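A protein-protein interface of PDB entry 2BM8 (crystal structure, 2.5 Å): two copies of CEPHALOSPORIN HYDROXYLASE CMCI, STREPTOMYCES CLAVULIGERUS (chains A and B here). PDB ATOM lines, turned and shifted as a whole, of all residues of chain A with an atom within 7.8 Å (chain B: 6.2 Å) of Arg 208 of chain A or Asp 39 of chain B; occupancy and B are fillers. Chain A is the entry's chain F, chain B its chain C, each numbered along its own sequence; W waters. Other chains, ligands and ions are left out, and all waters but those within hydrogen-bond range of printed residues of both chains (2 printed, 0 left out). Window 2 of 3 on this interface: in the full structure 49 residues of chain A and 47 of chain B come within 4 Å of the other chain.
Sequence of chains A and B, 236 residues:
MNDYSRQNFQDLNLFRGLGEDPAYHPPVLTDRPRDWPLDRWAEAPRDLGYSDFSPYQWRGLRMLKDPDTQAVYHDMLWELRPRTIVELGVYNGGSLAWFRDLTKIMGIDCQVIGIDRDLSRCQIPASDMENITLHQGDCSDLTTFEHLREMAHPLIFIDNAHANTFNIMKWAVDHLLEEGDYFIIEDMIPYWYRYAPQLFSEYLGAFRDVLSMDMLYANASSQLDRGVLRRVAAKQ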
ATOM      1  N   MET A 169     -18.296   1.992  12.389  1.00  0.00           N
ATOM      2  CA  MET A 169     -19.211   2.607  13.344  1.00  0.00           C
ATOM      3  C   MET A 169     -20.666   2.288  13.004  1.00  0.00           C
ATOM      4  O   MET A 169     -21.424   1.860  13.856  1.00  0.00           O
ATOM      5  CB  MET A 169     -19.026   4.124  13.319  1.00  0.00           C
ATOM      6  CG  MET A 169     -18.734   4.746  14.661  1.00  0.00           C
ATOM      7  SD  MET A 169     -18.161   6.452  14.436  1.00  0.00           S
ATOM      8  CE  MET A 169     -19.698   7.270  14.419  1.00  0.00           C
ATOM      9  N   SER A 201     -18.128  16.826  10.036  1.00  0.00           N
ATOM     10  CA  SER A 201     -19.306  17.250  10.795  1.00  0.00           C
ATOM     11  C   SER A 201     -20.586  16.563  10.313  1.00  0.00           C
ATOM     12  O   SER A 201     -21.418  16.169  11.118  1.00  0.00           O
ATOM     13  CB  SER A 201     -19.486  18.773  10.723  1.00  0.00           C
ATOM     14  OG  SER A 201     -18.515  19.401  11.539  1.00  0.00           O
ATOM     15  N   GLU A 202     -20.746  16.418   9.004  1.00  0.00           N
ATOM     16  CA  GLU A 202     -21.895  15.701   8.447  1.00  0.00           C
ATOM     17  C   GLU A 202     -21.852  14.231   8.905  1.00  0.00           C
ATOM     18  O   GLU A 202     -22.862  13.683   9.352  1.00  0.00           O
ATOM     19  CB  GLU A 202     -21.909  15.808   6.905  1.00  0.00           C
ATOM     20  CG  GLU A 202     -23.132  15.234   6.188  1.00  0.00           C
ATOM     21  CD  GLU A 202     -22.951  15.130   4.667  1.00  0.00           C
ATOM     22  OE1 GLU A 202     -23.966  15.052   3.928  1.00  0.00           O
ATOM     23  OE2 GLU A 202     -21.795  15.111   4.181  1.00  0.00           O
ATOM     24  N   TYR A 203     -20.681  13.602   8.832  1.00  0.00           N
ATOM     25  CA  TYR A 203     -20.613  12.159   9.081  1.00  0.00           C
ATOM     26  C   TYR A 203     -20.929  11.890  10.541  1.00  0.00           C
ATOM     27  O   TYR A 203     -21.818  11.113  10.834  1.00  0.00           O
ATOM     28  CB  TYR A 203     -19.260  11.574   8.697  1.00  0.00           C
ATOM     29  CG  TYR A 203     -18.998  11.464   7.211  1.00  0.00           C
ATOM     30  CD1 TYR A 203     -17.769  11.013   6.749  1.00  0.00           C
ATOM     31  CD2 TYR A 203     -19.964  11.798   6.272  1.00  0.00           C
ATOM     32  CE1 TYR A 203     -17.508  10.906   5.407  1.00  0.00           C
ATOM     33  CE2 TYR A 203     -19.704  11.695   4.910  1.00  0.00           C
ATOM     34  CZ  TYR A 203     -18.472  11.249   4.490  1.00  0.00           C
ATOM     35  OH  TYR A 203     -18.210  11.136   3.148  1.00  0.00           O
ATOM     36  N   LEU A 204     -20.226  12.574  11.439  1.00  0.00           N
ATOM     37  CA  LEU A 204     -20.431  12.417  12.876  1.00  0.00           C
ATOM     38  C   LEU A 204     -21.871  12.745  13.268  1.00  0.00           C
ATOM     39  O   LEU A 204     -22.477  12.024  14.027  1.00  0.00           O
ATOM     40  CB  LEU A 204     -19.468  13.320  13.682  1.00  0.00           C
ATOM     41  CG  LEU A 204     -18.533  12.724  14.738  1.00  0.00           C
ATOM     42  CD1 LEU A 204     -18.496  13.609  15.959  1.00  0.00           C
ATOM     43  CD2 LEU A 204     -18.847  11.302  15.136  1.00  0.00           C
ATOM     44  N   GLY A 205     -22.409  13.834  12.737  1.00  0.00           N
ATOM     45  CA  GLY A 205     -23.756  14.262  13.059  1.00  0.00           C
ATOM     46  C   GLY A 205     -24.847  13.324  12.573  1.00  0.00           C
ATOM     47  O   GLY A 205     -25.980  13.428  13.017  1.00  0.00           O
ATOM     48  N   ALA A 206     -24.522  12.427  11.648  1.00  0.00           N
ATOM     49  CA  ALA A 206     -25.478  11.441  11.146  1.00  0.00           C
ATOM     50  C   ALA A 206     -25.714  10.369  12.197  1.00  0.00           C
ATOM     51  O   ALA A 206     -26.730   9.679  12.145  1.00  0.00           O
ATOM     52  CB  ALA A 206     -24.964  10.802   9.853  1.00  0.00           C
ATOM     53  N   PHE A 207     -24.764  10.216  13.129  1.00  0.00           N
ATOM     54  CA  PHE A 207     -24.923   9.311  14.274  1.00  0.00           C
ATOM     55  C   PHE A 207     -25.565   9.982  15.502  1.00  0.00           C
ATOM     56  O   PHE A 207     -25.475   9.444  16.598  1.00  0.00           O
ATOM     57  CB  PHE A 207     -23.571   8.739  14.690  1.00  0.00           C
ATOM     58  CG  PHE A 207     -22.984   7.806  13.701  1.00  0.00           C
ATOM     59  CD1 PHE A 207     -22.209   8.284  12.669  1.00  0.00           C
ATOM     60  CD2 PHE A 207     -23.216   6.445  13.796  1.00  0.00           C
ATOM     61  CE1 PHE A 207     -21.674   7.419  11.748  1.00  0.00           C
ATOM     62  CE2 PHE A 207     -22.678   5.573  12.886  1.00  0.00           C
ATOM     63  CZ  PHE A 207     -21.905   6.056  11.858  1.00  0.00           C
ATOM     64  N   ARG A 208     -26.219  11.142  15.328  1.00  0.00           N
ATOM     65  CA  ARG A 208     -26.704  11.921  16.482  1.00  0.00           C
ATOM     66  C   ARG A 208     -27.774  11.203  17.317  1.00  0.00           C
ATOM     67  O   ARG A 208     -27.872  11.446  18.516  1.00  0.00           O
ATOM     68  CB  ARG A 208     -27.207  13.310  16.061  1.00  0.00           C
ATOM     69  CG  ARG A 208     -28.622  13.366  15.491  1.00  0.00           C
ATOM     70  CD  ARG A 208     -28.947  14.684  14.805  1.00  0.00           C
ATOM     71  NE  ARG A 208     -30.166  14.662  13.981  1.00  0.00           N
ATOM     72  CZ  ARG A 208     -30.244  14.203  12.725  1.00  0.00           C
ATOM     73  NH1 ARG A 208     -29.175  13.678  12.107  1.00  0.00           N
ATOM     74  NH2 ARG A 208     -31.410  14.256  12.083  1.00  0.00           N
ATOM     75  N   ASP A 209     -28.557  10.316  16.708  1.00  0.00           N
ATOM     76  CA  ASP A 209     -29.594   9.600  17.465  1.00  0.00           C
ATOM     77  C   ASP A 209     -29.127   8.343  18.187  1.00  0.00           C
ATOM     78  O   ASP A 209     -29.882   7.793  18.983  1.00  0.00           O
ATOM     79  CB  ASP A 209     -30.777   9.250  16.560  1.00  0.00           C
ATOM     80  CG  ASP A 209     -31.476  10.474  16.046  1.00  0.00           C
ATOM     81  OD1 ASP A 209     -31.983  11.256  16.878  1.00  0.00           O
ATOM     82  OD2 ASP A 209     -31.543  10.750  14.827  1.00  0.00           O
ATOM     83  N   VAL A 210     -27.903   7.896  17.913  1.00  0.00           N
ATOM     84  CA  VAL A 210     -27.419   6.602  18.402  1.00  0.00           C
ATOM     85  C   VAL A 210     -26.163   6.666  19.228  1.00  0.00           C
ATOM     86  O   VAL A 210     -25.939   5.782  20.049  1.00  0.00           O
ATOM     87  CB  VAL A 210     -27.164   5.621  17.259  1.00  0.00           C
ATOM     88  CG1 VAL A 210     -28.465   5.277  16.577  1.00  0.00           C
ATOM     89  CG2 VAL A 210     -26.174   6.182  16.249  1.00  0.00           C
ATOM     90  N   LEU A 211     -25.340   7.688  19.019  1.00  0.00           N
ATOM     91  CA  LEU A 211     -24.116   7.879  19.802  1.00  0.00           C
ATOM     92  C   LEU A 211     -23.991   9.310  20.291  1.00  0.00           C
ATOM     93  O   LEU A 211     -24.434  10.253  19.638  1.00  0.00           O
ATOM     94  CB  LEU A 211     -22.870   7.537  18.978  1.00  0.00           C
ATOM     95  CG  LEU A 211     -22.691   6.121  18.414  1.00  0.00           C
ATOM     96  CD1 LEU A 211     -21.515   6.116  17.457  1.00  0.00           C
ATOM     97  CD2 LEU A 211     -22.477   5.085  19.481  1.00  0.00           C
ATOM     98  N   SER A 212     -23.366   9.470  21.448  1.00  0.00           N
ATOM     99  CA  SER A 212     -23.096  10.787  21.986  1.00  0.00           C
ATOM    100  C   SER A 212     -21.659  10.860  22.437  1.00  0.00           C
ATOM    101  O   SER A 212     -21.013   9.844  22.646  1.00  0.00           O
ATOM    102  CB  SER A 212     -24.050  11.094  23.145  1.00  0.00           C
ATOM    103  OG  SER A 212     -23.530  10.642  24.381  1.00  0.00           O
ATOM    104  N   VAL A 232     -26.252   5.640  23.192  1.00  0.00           N
ATOM    105  CA  VAL A 232     -27.337   6.231  23.958  1.00  0.00           C
ATOM    106  C   VAL A 232     -28.562   5.315  23.851  1.00  0.00           C
ATOM    107  O   VAL A 232     -28.619   4.430  22.992  1.00  0.00           O
ATOM    108  CB  VAL A 232     -27.601   7.684  23.442  1.00  0.00           C
ATOM    109  CG1 VAL A 232     -28.984   8.216  23.803  1.00  0.00           C
ATOM    110  CG2 VAL A 232     -26.545   8.618  23.991  1.00  0.00           C
ATOM    111  N   ALA A 233     -29.514   5.491  24.761  1.00  0.00           N
ATOM    112  CA  ALA A 233     -30.808   4.794  24.694  1.00  0.00           C
ATOM    113  C   ALA A 233     -31.589   5.190  23.452  1.00  0.00           C
ATOM    114  O   ALA A 233     -31.573   6.350  23.057  1.00  0.00           O
ATOM    115  CB  ALA A 233     -31.640   5.108  25.950  1.00  0.00           C
ATOM    116  N   PRO B  37     -24.618  16.007  22.253  1.00  0.00           N
ATOM    117  CA  PRO B  37     -25.195  15.553  20.993  1.00  0.00           C
ATOM    118  C   PRO B  37     -24.217  15.756  19.834  1.00  0.00           C
ATOM    119  O   PRO B  37     -23.559  16.786  19.741  1.00  0.00           O
ATOM    120  CB  PRO B  37     -26.450  16.430  20.844  1.00  0.00           C
ATOM    121  CG  PRO B  37     -26.143  17.656  21.607  1.00  0.00           C
ATOM    122  CD  PRO B  37     -25.289  17.213  22.761  1.00  0.00           C
ATOM    123  N   LEU B  38     -24.176  14.791  18.933  1.00  0.00           N
ATOM    124  CA  LEU B  38     -23.099  14.683  17.957  1.00  0.00           C
ATOM    125  C   LEU B  38     -23.264  15.623  16.757  1.00  0.00           C
ATOM    126  O   LEU B  38     -22.275  15.982  16.118  1.00  0.00           O
ATOM    127  CB  LEU B  38     -23.002  13.239  17.493  1.00  0.00           C
ATOM    128  CG  LEU B  38     -21.751  12.458  17.878  1.00  0.00           C
ATOM    129  CD1 LEU B  38     -21.161  12.833  19.213  1.00  0.00           C
ATOM    130  CD2 LEU B  38     -22.003  10.950  17.790  1.00  0.00           C
ATOM    131  N   ASP B  39     -24.498  16.017  16.455  1.00  0.00           N
ATOM    132  CA  ASP B  39     -24.741  17.055  15.470  1.00  0.00           C
ATOM    133  C   ASP B  39     -24.360  18.458  15.942  1.00  0.00           C
ATOM    134  O   ASP B  39     -24.457  19.414  15.183  1.00  0.00           O
ATOM    135  CB  ASP B  39     -26.217  17.042  14.979  1.00  0.00           C
ATOM    136  CG  ASP B  39     -27.231  17.455  16.058  1.00  0.00           C
ATOM    137  OD1 ASP B  39     -27.116  17.059  17.227  1.00  0.00           O
ATOM    138  OD2 ASP B  39     -28.229  18.150  15.808  1.00  0.00           O
ATOM    139  N   ARG B  40     -23.953  18.596  17.198  1.00  0.00           N
ATOM    140  CA  ARG B  40     -23.393  19.855  17.682  1.00  0.00           C
ATOM    141  C   ARG B  40     -22.000  19.620  18.230  1.00  0.00           C
ATOM    142  O   ARG B  40     -21.520  20.364  19.080  1.00  0.00           O
ATOM    143  CB  ARG B  40     -24.304  20.461  18.744  1.00  0.00           C
ATOM    144  CG  ARG B  40     -25.751  20.631  18.286  1.00  0.00           C
ATOM    145  CD  ARG B  40     -25.929  21.690  17.209  1.00  0.00           C
ATOM    146  NE  ARG B  40     -25.967  23.028  17.805  1.00  0.00           N
ATOM    147  CZ  ARG B  40     -26.951  23.916  17.645  1.00  0.00           C
ATOM    148  NH1 ARG B  40     -28.021  23.652  16.892  1.00  0.00           N
ATOM    149  NH2 ARG B  40     -26.860  25.089  18.261  1.00  0.00           N
ATOM    150  N   TRP B  41     -21.335  18.601  17.704  1.00  0.00           N
ATOM    151  CA  TRP B  41     -20.032  18.189  18.212  1.00  0.00           C
ATOM    152  C   TRP B  41     -19.062  19.369  18.360  1.00  0.00           C
ATOM    153  O   TRP B  41     -18.463  19.548  19.420  1.00  0.00           O
ATOM    154  CB  TRP B  41     -19.460  17.111  17.295  1.00  0.00           C
ATOM    155  CG  TRP B  41     -18.085  16.698  17.608  1.00  0.00           C
ATOM    156  CD1 TRP B  41     -17.697  15.754  18.505  1.00  0.00           C
ATOM    157  CD2 TRP B  41     -16.902  17.185  16.998  1.00  0.00           C
ATOM    158  NE1 TRP B  41     -16.335  15.640  18.500  1.00  0.00           N
ATOM    159  CE2 TRP B  41     -15.823  16.506  17.574  1.00  0.00           C
ATOM    160  CE3 TRP B  41     -16.644  18.139  16.009  1.00  0.00           C
ATOM    161  CZ2 TRP B  41     -14.501  16.747  17.206  1.00  0.00           C
ATOM    162  CZ3 TRP B  41     -15.336  18.378  15.646  1.00  0.00           C
ATOM    163  CH2 TRP B  41     -14.279  17.683  16.247  1.00  0.00           C
ATOM    164  N   ALA B  42     -18.972  20.197  17.315  1.00  0.00           N
ATOM    165  CA  ALA B  42     -17.992  21.286  17.226  1.00  0.00           C
ATOM    166  C   ALA B  42     -18.164  22.377  18.256  1.00  0.00           C
ATOM    167  O   ALA B  42     -17.244  23.134  18.490  1.00  0.00           O
ATOM    168  CB  ALA B  42     -18.027  21.919  15.839  1.00  0.00           C
ATOM    169  N   GLU B  43     -19.346  22.487  18.848  1.00  0.00           N
ATOM    170  CA  GLU B  43     -19.606  23.530  19.820  1.00  0.00           C
ATOM    171  C   GLU B  43     -19.442  23.055  21.260  1.00  0.00           C
ATOM    172  O   GLU B  43     -19.802  23.771  22.183  1.00  0.00           O
ATOM    173  CB  GLU B  43     -21.015  24.089  19.586  1.00  0.00           C
ATOM    174  CG  GLU B  43     -21.163  24.798  18.253  1.00  0.00           C
ATOM    175  CD  GLU B  43     -22.595  24.810  17.756  1.00  0.00           C
ATOM    176  OE1 GLU B  43     -23.127  23.735  17.395  1.00  0.00           O
ATOM    177  OE2 GLU B  43     -23.200  25.900  17.715  1.00  0.00           O
HETATM  178  O   HOH W   1     -21.270  16.951  14.014  1.00  0.00           O
HETATM  179  O   HOH W   2     -25.630  12.371  19.896  1.00  0.00           O
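The backbone carbonyl oxygen of Gly 205 of chain A lies close to the guanidinium group of Arg 208 of chain A (3.3 Å).
Water W2 lies within hydrogen-bond range of O of Leu 211 of chain A (2.4 Å), O of Arg 208 of chain A (2.8 Å) and N of Leu 38 of chain B (3.0 Å). Water W1 bridges O of Leu 38 of chain B and O of Ser 201 of chain A.
Of chain A, only Gly 205 (3.8 Å) and Arg 208 (3.5 Å) come within 4 Å of Asp 39 of chain B. Of the printed residues of chain B, Ser 212 of chain A touches Leu 38. Of the printed residues of chain B, Leu 211 of chain A touches Leu 38. Of the printed residues of chain B, Gly 205 of chain A touches Leu 38 (3.8 Å) and Asp 39 (3.8 Å). Of the printed residues of chain B, Leu 204 of chain A touches Leu 38 and Trp 41. Printed residues of chain B within 4 Å of Phe 207 of chain A: Leu 38. Asp 209 of chain A touches none of the printed residues of chain B. Ala 206 of chain A touches none of the printed residues of chain B. The nearest residue of chain B that does not touch Arg 208 of chain A is Leu 38 of chain B (4.1 Å). The nearest residue of chain A that does not touch Asp 39 of chain B is Leu 204 of chain A (5.1 Å).
Leu 38 of chain B touches Leu 204 of chain A. CD1 of Trp 41 of chain B touches CD1 of Leu 204 of chain A, at 3.4 Å. Gly 205 of chain A touches Leu 38 of chain B. CA of Gly 205 of chain A touches CA of Asp 39 of chain B (3.8 Å). O of Phe 207 of chain A touches CD2 of Leu 38 of chain B, 3.97 Å away. Asp 39 of chain B touches Arg 208 of chain A. Leu 211 of chain A touches Leu 38 of chain B. C of Ser 212 of chain A touches CD1 of Leu 38 of chain B, 3.8 Å away.
No position is printed for both chains.
Hydrophobic or aromatic side chains of chain B within 4 Å of the printed part of chain A: Leu 38 and Trp 41. Among the printed residues, no Asp or Glu carboxylate lies within 4 Å of a Lys or Arg side-chain nitrogen of the other chain.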
